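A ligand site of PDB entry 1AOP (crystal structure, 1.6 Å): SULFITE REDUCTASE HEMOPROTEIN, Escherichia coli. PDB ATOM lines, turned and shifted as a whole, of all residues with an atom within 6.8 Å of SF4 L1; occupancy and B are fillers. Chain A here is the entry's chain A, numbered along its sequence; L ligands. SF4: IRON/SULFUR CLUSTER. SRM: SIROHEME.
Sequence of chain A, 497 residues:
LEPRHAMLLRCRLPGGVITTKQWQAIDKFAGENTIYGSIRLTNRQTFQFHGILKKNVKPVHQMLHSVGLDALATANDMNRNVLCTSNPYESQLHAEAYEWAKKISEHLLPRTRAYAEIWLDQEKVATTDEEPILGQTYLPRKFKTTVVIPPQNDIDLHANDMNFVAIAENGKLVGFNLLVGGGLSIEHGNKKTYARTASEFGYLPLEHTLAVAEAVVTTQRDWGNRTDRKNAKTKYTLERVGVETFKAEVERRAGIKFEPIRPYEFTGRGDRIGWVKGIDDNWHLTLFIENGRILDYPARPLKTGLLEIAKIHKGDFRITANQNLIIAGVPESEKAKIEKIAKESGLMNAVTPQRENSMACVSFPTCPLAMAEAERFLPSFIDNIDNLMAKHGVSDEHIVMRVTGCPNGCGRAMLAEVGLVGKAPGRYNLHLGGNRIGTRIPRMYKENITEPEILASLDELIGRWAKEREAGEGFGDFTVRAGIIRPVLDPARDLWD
The backbone NH (N) of Cys 410 lies close to a sulfur (S2) of SF4 L1 (3.4 Å).
An iron atom (FE4) of SF4 L1 is bound by the side-chain sulfur (SG) of Cys 410, 2.2 Å away.
FE2 of SF4 L1 is bound by SG of Cys 367, at 2.2 Å.
SG of Cys 361 binds FE1 of SF4 L1, 2.2 Å away.
The side-chain sulfur (SG) of Cys 406 binds an iron atom (FE3) of SF4 L1.
A sulfur (S2) of SF4 L1 lies close to the side-chain hydroxyl (OG1) of Thr 404 (3.1 Å).
A sulfur (S1) of SF4 L1 sits close to the side-chain amide nitrogen (ND2) of Asn 408 (3.6 Å).
A sulfur (S3) of SF4 L1 sits close to the backbone NH (N) of Ser 363 (3.8 Å).
The backbone NH of Gly 409 sits close to a sulfur (S2) of SF4 L1 (3.8 Å).
The backbone NH of Cys 367 is in hydrogen-bond range of an oxygen (O1A) of SRM L2.
N of Val 362 lies within hydrogen-bond range of O3B of SRM L2.
Merely in contact with SF4 L1: Ala 370, Gly 405 and Leu 369.
Hydrophobic or aromatic side chains within 4 Å of SF4 L1: Leu 369 and Ala 370.
11 residues have an atom within 4 Å of SF4 L1: Cys 361, Ser 363, Cys 367, Leu 369, Ala 370, Thr 404, Gly 405, Cys 406, Asn 408, Gly 409 and Cys 410.
The nearest printed residue that does not touch SF4 L1 is Val 362 (4.1 Å).
The side-chain sulfur (SG) of Cys 367 sits close to the backbone NH (N) of Leu 369.
The side-chain sulfur (SG) of Cys 361 lies close to the backbone NH (N) of Gly 405 (3.2 Å).
ND2 of Asn 408 sits close to SG of Cys 406, at 3.4 Å.
SG of Cys 406 lies close to O of Leu 369 (3.8 Å).
N of Gly 411 sits at hydrogen-bond distance from OG1 of Thr 404, 3.1 Å away.
O of Gly 405 lies within hydrogen-bond range of N of Met 371 (3.0 Å).
The backbone carbonyl oxygen of Gly 405 sits at hydrogen-bond distance from the backbone NH of Ala 372 (3.1 Å).
The side-chain hydroxyl of Ser 363 is in hydrogen-bond range of the backbone carbonyl oxygen of Ala 372, at 2.7 Å.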
ATOM      1  N   ALA A 360     -18.117  -7.454  11.038  1.00  0.00           N
ATOM      2  CA  ALA A 360     -17.358  -6.197  11.180  1.00  0.00           C
ATOM      3  C   ALA A 360     -18.177  -5.189  11.990  1.00  0.00           C
ATOM      4  O   ALA A 360     -19.413  -5.262  12.023  1.00  0.00           O
ATOM      5  CB  ALA A 360     -17.049  -5.606   9.790  1.00  0.00           C
ATOM      6  N   CYS A 361     -17.500  -4.252  12.646  1.00  0.00           N
ATOM      7  CA  CYS A 361     -18.184  -3.197  13.407  1.00  0.00           C
ATOM      8  C   CYS A 361     -18.521  -2.036  12.450  1.00  0.00           C
ATOM      9  O   CYS A 361     -18.071  -2.030  11.300  1.00  0.00           O
ATOM     10  CB  CYS A 361     -17.275  -2.685  14.532  1.00  0.00           C
ATOM     11  SG  CYS A 361     -15.886  -1.684  13.893  1.00  0.00           S
ATOM     12  N   VAL A 362     -19.301  -1.067  12.935  1.00  0.00           N
ATOM     13  CA  VAL A 362     -19.695   0.098  12.135  1.00  0.00           C
ATOM     14  C   VAL A 362     -18.500   0.901  11.590  1.00  0.00           C
ATOM     15  O   VAL A 362     -18.373   1.110  10.380  1.00  0.00           O
ATOM     16  CB  VAL A 362     -20.632   1.045  12.928  1.00  0.00           C
ATOM     17  CG1 VAL A 362     -20.942   2.302  12.100  1.00  0.00           C
ATOM     18  CG2 VAL A 362     -21.939   0.333  13.322  1.00  0.00           C
ATOM     19  N   SER A 363     -17.620   1.355  12.501  1.00  0.00           N
ATOM     20  CA  SER A 363     -16.443   2.149  12.098  1.00  0.00           C
ATOM     21  C   SER A 363     -16.871   3.383  11.251  1.00  0.00           C
ATOM     22  O   SER A 363     -17.926   3.975  11.514  1.00  0.00           O
ATOM     23  CB  SER A 363     -15.459   1.267  11.315  1.00  0.00           C
ATOM     24  OG  SER A 363     -14.247   1.949  11.062  1.00  0.00           O
ATOM     25  N   PHE A 364     -16.062   3.776  10.259  1.00  0.00           N
ATOM     26  CA  PHE A 364     -16.403   4.923   9.412  1.00  0.00           C
ATOM     27  C   PHE A 364     -17.703   4.623   8.651  1.00  0.00           C
ATOM     28  O   PHE A 364     -17.941   3.490   8.254  1.00  0.00           O
ATOM     29  CB  PHE A 364     -15.270   5.184   8.411  1.00  0.00           C
ATOM     30  CG  PHE A 364     -13.970   5.554   9.042  1.00  0.00           C
ATOM     31  CD1 PHE A 364     -13.832   6.748   9.741  1.00  0.00           C
ATOM     32  CD2 PHE A 364     -12.869   4.709   8.913  1.00  0.00           C
ATOM     33  CE1 PHE A 364     -12.602   7.105  10.302  1.00  0.00           C
ATOM     34  CE2 PHE A 364     -11.631   5.060   9.472  1.00  0.00           C
ATOM     35  CZ  PHE A 364     -11.501   6.262  10.162  1.00  0.00           C
ATOM     36  N   CYS A 367     -18.482   6.348  13.263  1.00  0.00           N
ATOM     37  CA  CYS A 367     -17.781   6.168  14.531  1.00  0.00           C
ATOM     38  C   CYS A 367     -16.654   7.169  14.699  1.00  0.00           C
ATOM     39  O   CYS A 367     -15.707   7.192  13.926  1.00  0.00           O
ATOM     40  CB  CYS A 367     -17.238   4.759  14.697  1.00  0.00           C
ATOM     41  SG  CYS A 367     -16.553   4.540  16.366  1.00  0.00           S
ATOM     42  N   PRO A 368     -16.697   7.948  15.786  1.00  0.00           N
ATOM     43  CA  PRO A 368     -15.640   8.942  16.007  1.00  0.00           C
ATOM     44  C   PRO A 368     -14.308   8.375  16.449  1.00  0.00           C
ATOM     45  O   PRO A 368     -13.306   9.094  16.457  1.00  0.00           O
ATOM     46  CB  PRO A 368     -16.266   9.847  17.063  1.00  0.00           C
ATOM     47  CG  PRO A 368     -17.080   8.902  17.879  1.00  0.00           C
ATOM     48  CD  PRO A 368     -17.741   8.042  16.809  1.00  0.00           C
ATOM     49  N   LEU A 369     -14.296   7.101  16.839  1.00  0.00           N
ATOM     50  CA  LEU A 369     -13.076   6.447  17.331  1.00  0.00           C
ATOM     51  C   LEU A 369     -12.383   5.525  16.309  1.00  0.00           C
ATOM     52  O   LEU A 369     -11.367   4.911  16.604  1.00  0.00           O
ATOM     53  CB  LEU A 369     -13.415   5.646  18.611  1.00  0.00           C
ATOM     54  CG  LEU A 369     -14.289   6.332  19.668  1.00  0.00           C
ATOM     55  CD1 LEU A 369     -14.552   5.374  20.813  1.00  0.00           C
ATOM     56  CD2 LEU A 369     -13.618   7.584  20.169  1.00  0.00           C
ATOM     57  N   ALA A 370     -12.945   5.446  15.108  1.00  0.00           N
ATOM     58  CA  ALA A 370     -12.427   4.581  14.054  1.00  0.00           C
ATOM     59  C   ALA A 370     -10.989   4.861  13.592  1.00  0.00           C
ATOM     60  O   ALA A 370     -10.585   6.027  13.407  1.00  0.00           O
ATOM     61  CB  ALA A 370     -13.359   4.607  12.849  1.00  0.00           C
ATOM     62  N   MET A 371     -10.221   3.781  13.403  1.00  0.00           N
ATOM     63  CA  MET A 371      -8.852   3.878  12.920  1.00  0.00           C
ATOM     64  C   MET A 371      -8.777   3.340  11.490  1.00  0.00           C
ATOM     65  O   MET A 371      -8.049   3.878  10.661  1.00  0.00           O
ATOM     66  CB  MET A 371      -7.889   3.118  13.832  1.00  0.00           C
ATOM     67  CG  MET A 371      -7.792   3.696  15.251  1.00  0.00           C
ATOM     68  SD  MET A 371      -6.718   2.684  16.314  1.00  0.00           S
ATOM     69  CE  MET A 371      -6.776   3.591  17.925  1.00  0.00           C
ATOM     70  N   ALA A 372      -9.530   2.290  11.193  1.00  0.00           N
ATOM     71  CA  ALA A 372      -9.543   1.728   9.844  1.00  0.00           C
ATOM     72  C   ALA A 372     -10.966   1.300   9.513  1.00  0.00           C
ATOM     73  O   ALA A 372     -11.774   1.105  10.421  1.00  0.00           O
ATOM     74  CB  ALA A 372      -8.579   0.555   9.741  1.00  0.00           C
ATOM     75  N   ALA A 374     -14.169  -0.898   8.593  1.00  0.00           N
ATOM     76  CA  ALA A 374     -14.568  -2.242   9.019  1.00  0.00           C
ATOM     77  C   ALA A 374     -15.782  -2.628   8.177  1.00  0.00           C
ATOM     78  O   ALA A 374     -15.644  -3.368   7.195  1.00  0.00           O
ATOM     79  CB  ALA A 374     -14.865  -2.276  10.524  1.00  0.00           C
ATOM     80  N   VAL A 403     -13.511  -8.300  11.562  1.00  0.00           N
ATOM     81  CA  VAL A 403     -12.780  -7.032  11.442  1.00  0.00           C
ATOM     82  C   VAL A 403     -13.329  -5.994  12.408  1.00  0.00           C
ATOM     83  O   VAL A 403     -14.526  -5.719  12.413  1.00  0.00           O
ATOM     84  CB  VAL A 403     -12.918  -6.473  10.006  1.00  0.00           C
ATOM     85  CG1 VAL A 403     -12.039  -5.228   9.834  1.00  0.00           C
ATOM     86  CG2 VAL A 403     -12.546  -7.527   9.004  1.00  0.00           C
ATOM     87  N   THR A 404     -12.475  -5.436  13.248  1.00  0.00           N
ATOM     88  CA  THR A 404     -12.901  -4.406  14.176  1.00  0.00           C
ATOM     89  C   THR A 404     -12.077  -3.153  13.805  1.00  0.00           C
ATOM     90  O   THR A 404     -10.879  -3.252  13.537  1.00  0.00           O
ATOM     91  CB  THR A 404     -12.780  -4.909  15.645  1.00  0.00           C
ATOM     92  OG1 THR A 404     -13.554  -4.066  16.513  1.00  0.00           O
ATOM     93  CG2 THR A 404     -11.324  -4.947  16.110  1.00  0.00           C
ATOM     94  N   GLY A 405     -12.759  -2.011  13.686  1.00  0.00           N
ATOM     95  CA  GLY A 405     -12.117  -0.747  13.285  1.00  0.00           C
ATOM     96  C   GLY A 405     -11.067  -0.114  14.181  1.00  0.00           C
ATOM     97  O   GLY A 405     -10.320   0.759  13.742  1.00  0.00           O
ATOM     98  N   CYS A 406     -11.053  -0.507  15.441  1.00  0.00           N
ATOM     99  CA  CYS A 406     -10.086  -0.014  16.417  1.00  0.00           C
ATOM    100  C   CYS A 406     -10.016  -1.069  17.528  1.00  0.00           C
ATOM    101  O   CYS A 406     -10.847  -1.980  17.567  1.00  0.00           O
ATOM    102  CB  CYS A 406     -10.450   1.409  16.927  1.00  0.00           C
ATOM    103  SG  CYS A 406     -11.730   1.522  18.200  1.00  0.00           S
ATOM    104  N   PRO A 407      -9.074  -0.925  18.469  1.00  0.00           N
ATOM    105  CA  PRO A 407      -8.972  -1.923  19.539  1.00  0.00           C
ATOM    106  C   PRO A 407     -10.082  -2.022  20.590  1.00  0.00           C
ATOM    107  O   PRO A 407     -10.072  -2.962  21.400  1.00  0.00           O
ATOM    108  CB  PRO A 407      -7.592  -1.641  20.130  1.00  0.00           C
ATOM    109  CG  PRO A 407      -7.510  -0.144  20.022  1.00  0.00           C
ATOM    110  CD  PRO A 407      -8.068   0.149  18.647  1.00  0.00           C
ATOM    111  N   ASN A 408     -11.041  -1.095  20.576  1.00  0.00           N
ATOM    112  CA  ASN A 408     -12.176  -1.145  21.505  1.00  0.00           C
ATOM    113  C   ASN A 408     -12.854  -2.492  21.333  1.00  0.00           C
ATOM    114  O   ASN A 408     -13.483  -3.015  22.251  1.00  0.00           O
ATOM    115  CB  ASN A 408     -13.118   0.040  21.274  1.00  0.00           C
ATOM    116  CG  ASN A 408     -12.595   1.325  21.921  1.00  0.00           C
ATOM    117  OD1 ASN A 408     -11.929   1.292  22.964  1.00  0.00           O
ATOM    118  ND2 ASN A 408     -12.894   2.456  21.304  1.00  0.00           N
ATOM    119  N   GLY A 409     -12.727  -3.024  20.105  1.00  0.00           N
ATOM    120  CA  GLY A 409     -13.201  -4.362  19.802  1.00  0.00           C
ATOM    121  C   GLY A 409     -14.642  -4.717  19.567  1.00  0.00           C
ATOM    122  O   GLY A 409     -14.989  -5.890  19.687  1.00  0.00           O
ATOM    123  N   CYS A 410     -15.457  -3.744  19.148  1.00  0.00           N
ATOM    124  CA  CYS A 410     -16.888  -3.956  18.898  1.00  0.00           C
ATOM    125  C   CYS A 410     -17.209  -5.070  17.897  1.00  0.00           C
ATOM    126  O   CYS A 410     -18.255  -5.690  18.012  1.00  0.00           O
ATOM    127  CB  CYS A 410     -17.558  -2.660  18.452  1.00  0.00           C
ATOM    128  SG  CYS A 410     -17.129  -1.215  19.470  1.00  0.00           S
ATOM    129  N   GLY A 411     -16.327  -5.302  16.916  1.00  0.00           N
ATOM    130  CA  GLY A 411     -16.565  -6.355  15.933  1.00  0.00           C
ATOM    131  C   GLY A 411     -16.248  -7.757  16.458  1.00  0.00           C
ATOM    132  O   GLY A 411     -16.348  -8.722  15.709  1.00  0.00           O
HETATM  133 FE1  SF4 L   1     -15.486  -0.155  15.458  1.00  0.00          FE
HETATM  134 FE2  SF4 L   1     -16.007   2.407  16.467  1.00  0.00          FE
HETATM  135 FE3  SF4 L   1     -13.688   1.066  17.246  1.00  0.00          FE
HETATM  136 FE4  SF4 L   1     -16.230   0.147  18.056  1.00  0.00          FE
HETATM  137  S1  SF4 L   1     -15.322   2.103  18.680  1.00  0.00           S
HETATM  138  S2  SF4 L   1     -14.357  -1.139  17.277  1.00  0.00           S
HETATM  139  S3  SF4 L   1     -17.540   0.684  16.191  1.00  0.00           S
HETATM  140  S4  SF4 L   1     -14.234   1.725  15.063  1.00  0.00           S
HETATM  141 FE   SRM L   2     -19.386  -0.708  21.117  1.00  0.00          FE
HETATM  142  CHA SRM L   2     -18.046   2.351  21.746  1.00  0.00           C
HETATM  143  CHB SRM L   2     -20.631   0.520  18.106  1.00  0.00           C
HETATM  144  CHC SRM L   2     -20.692  -3.720  20.423  1.00  0.00           C
HETATM  145  CHD SRM L   2     -16.899  -2.187  22.963  1.00  0.00           C
HETATM  146  NA  SRM L   2     -19.478   1.184  20.155  1.00  0.00           N
HETATM  147  C1A SRM L   2     -18.935   2.351  20.677  1.00  0.00           C
HETATM  148  C2A SRM L   2     -19.456   3.546  19.868  1.00  0.00           C
HETATM  149  CMA SRM L   2     -20.763   3.933  20.623  1.00  0.00           C
HETATM  150  CDA SRM L   2     -18.430   4.726  19.677  1.00  0.00           C
HETATM  151  CEA SRM L   2     -18.463   5.854  20.708  1.00  0.00           C
HETATM  152  O3A SRM L   2     -18.292   5.580  21.911  1.00  0.00           O
HETATM  153  O4A SRM L   2     -18.672   7.021  20.317  1.00  0.00           O
HETATM  154  C3A SRM L   2     -19.668   2.891  18.521  1.00  0.00           C
HETATM  155  CAA SRM L   2     -20.690   3.536  17.661  1.00  0.00           C
HETATM  156  CBA SRM L   2     -20.420   3.402  16.166  1.00  0.00           C
HETATM  157  CCA SRM L   2     -21.539   3.990  15.321  1.00  0.00           C
HETATM  158  O1A SRM L   2     -21.332   5.057  14.688  1.00  0.00           O
HETATM  159  O2A SRM L   2     -22.624   3.376  15.265  1.00  0.00           O
HETATM  160  C4A SRM L   2     -20.031   1.462  18.929  1.00  0.00           C
HETATM  161  NB  SRM L   2     -20.516  -1.426  19.546  1.00  0.00           N
HETATM  162  C1B SRM L   2     -20.889  -0.813  18.375  1.00  0.00           C
HETATM  163  C2B SRM L   2     -21.830  -1.698  17.558  1.00  0.00           C
HETATM  164  CMB SRM L   2     -22.970  -0.854  16.843  1.00  0.00           C
HETATM  165  CDB SRM L   2     -20.964  -2.492  16.593  1.00  0.00           C
HETATM  166  CEB SRM L   2     -21.664  -3.255  15.482  1.00  0.00           C
HETATM  167  O3B SRM L   2     -21.205  -3.132  14.333  1.00  0.00           O
HETATM  168  O4B SRM L   2     -22.632  -3.981  15.757  1.00  0.00           O
HETATM  169  C3B SRM L   2     -22.314  -2.664  18.661  1.00  0.00           C
HETATM  170  CAB SRM L   2     -23.505  -2.035  19.395  1.00  0.00           C
HETATM  171  CBB SRM L   2     -24.039  -3.007  20.448  1.00  0.00           C
HETATM  172  CCB SRM L   2     -25.221  -2.430  21.234  1.00  0.00           C
HETATM  173  O1B SRM L   2     -26.345  -2.408  20.699  1.00  0.00           O
HETATM  174  O2B SRM L   2     -25.001  -2.000  22.395  1.00  0.00           O
HETATM  175  C4B SRM L   2     -21.090  -2.695  19.586  1.00  0.00           C
HETATM  176  NC  SRM L   2     -18.856  -2.672  21.637  1.00  0.00           N
HETATM  177  C1C SRM L   2     -19.635  -3.741  21.338  1.00  0.00           C
HETATM  178  C2C SRM L   2     -18.862  -4.890  21.727  1.00  0.00           C
HETATM  179  CDC SRM L   2     -19.299  -6.319  21.435  1.00  0.00           C
HETATM  180  CEC SRM L   2     -20.413  -6.859  22.312  1.00  0.00           C
HETATM  181  O3C SRM L   2     -20.797  -6.190  23.292  1.00  0.00           O
HETATM  182  O4C SRM L   2     -20.920  -7.964  22.024  1.00  0.00           O
HETATM  183  C3C SRM L   2     -17.724  -4.495  22.381  1.00  0.00           C
HETATM  184  CAC SRM L   2     -16.573  -5.378  22.822  1.00  0.00           C
HETATM  185  CBC SRM L   2     -16.806  -6.169  24.110  1.00  0.00           C
HETATM  186  CCC SRM L   2     -16.484  -5.368  25.367  1.00  0.00           C
HETATM  187  O1C SRM L   2     -17.236  -4.448  25.719  1.00  0.00           O
HETATM  188  O2C SRM L   2     -15.461  -5.669  26.007  1.00  0.00           O
HETATM  189  C4C SRM L   2     -17.779  -3.072  22.347  1.00  0.00           C
HETATM  190  ND  SRM L   2     -17.825  -0.018  22.316  1.00  0.00           N
HETATM  191  C1D SRM L   2     -16.919  -0.798  22.983  1.00  0.00           C
HETATM  192  C2D SRM L   2     -15.996   0.052  23.702  1.00  0.00           C
HETATM  193  CAD SRM L   2     -14.842  -0.405  24.581  1.00  0.00           C
HETATM  194  CBD SRM L   2     -15.360  -0.577  25.999  1.00  0.00           C
HETATM  195  CCD SRM L   2     -14.289  -0.922  27.015  1.00  0.00           C
HETATM  196  O1D SRM L   2     -14.580  -1.736  27.923  1.00  0.00           O
HETATM  197  O2D SRM L   2     -13.162  -0.390  26.931  1.00  0.00           O
HETATM  198  C3D SRM L   2     -16.356   1.349  23.333  1.00  0.00           C
HETATM  199  CDD SRM L   2     -15.659   2.648  23.730  1.00  0.00           C
HETATM  200  CED SRM L   2     -16.010   3.155  25.116  1.00  0.00           C
HETATM  201  O3D SRM L   2     -17.071   2.776  25.664  1.00  0.00           O
HETATM  202  O4D SRM L   2     -15.237   3.952  25.679  1.00  0.00           O
HETATM  203  C4D SRM L   2     -17.508   1.303  22.491  1.00  0.00           C
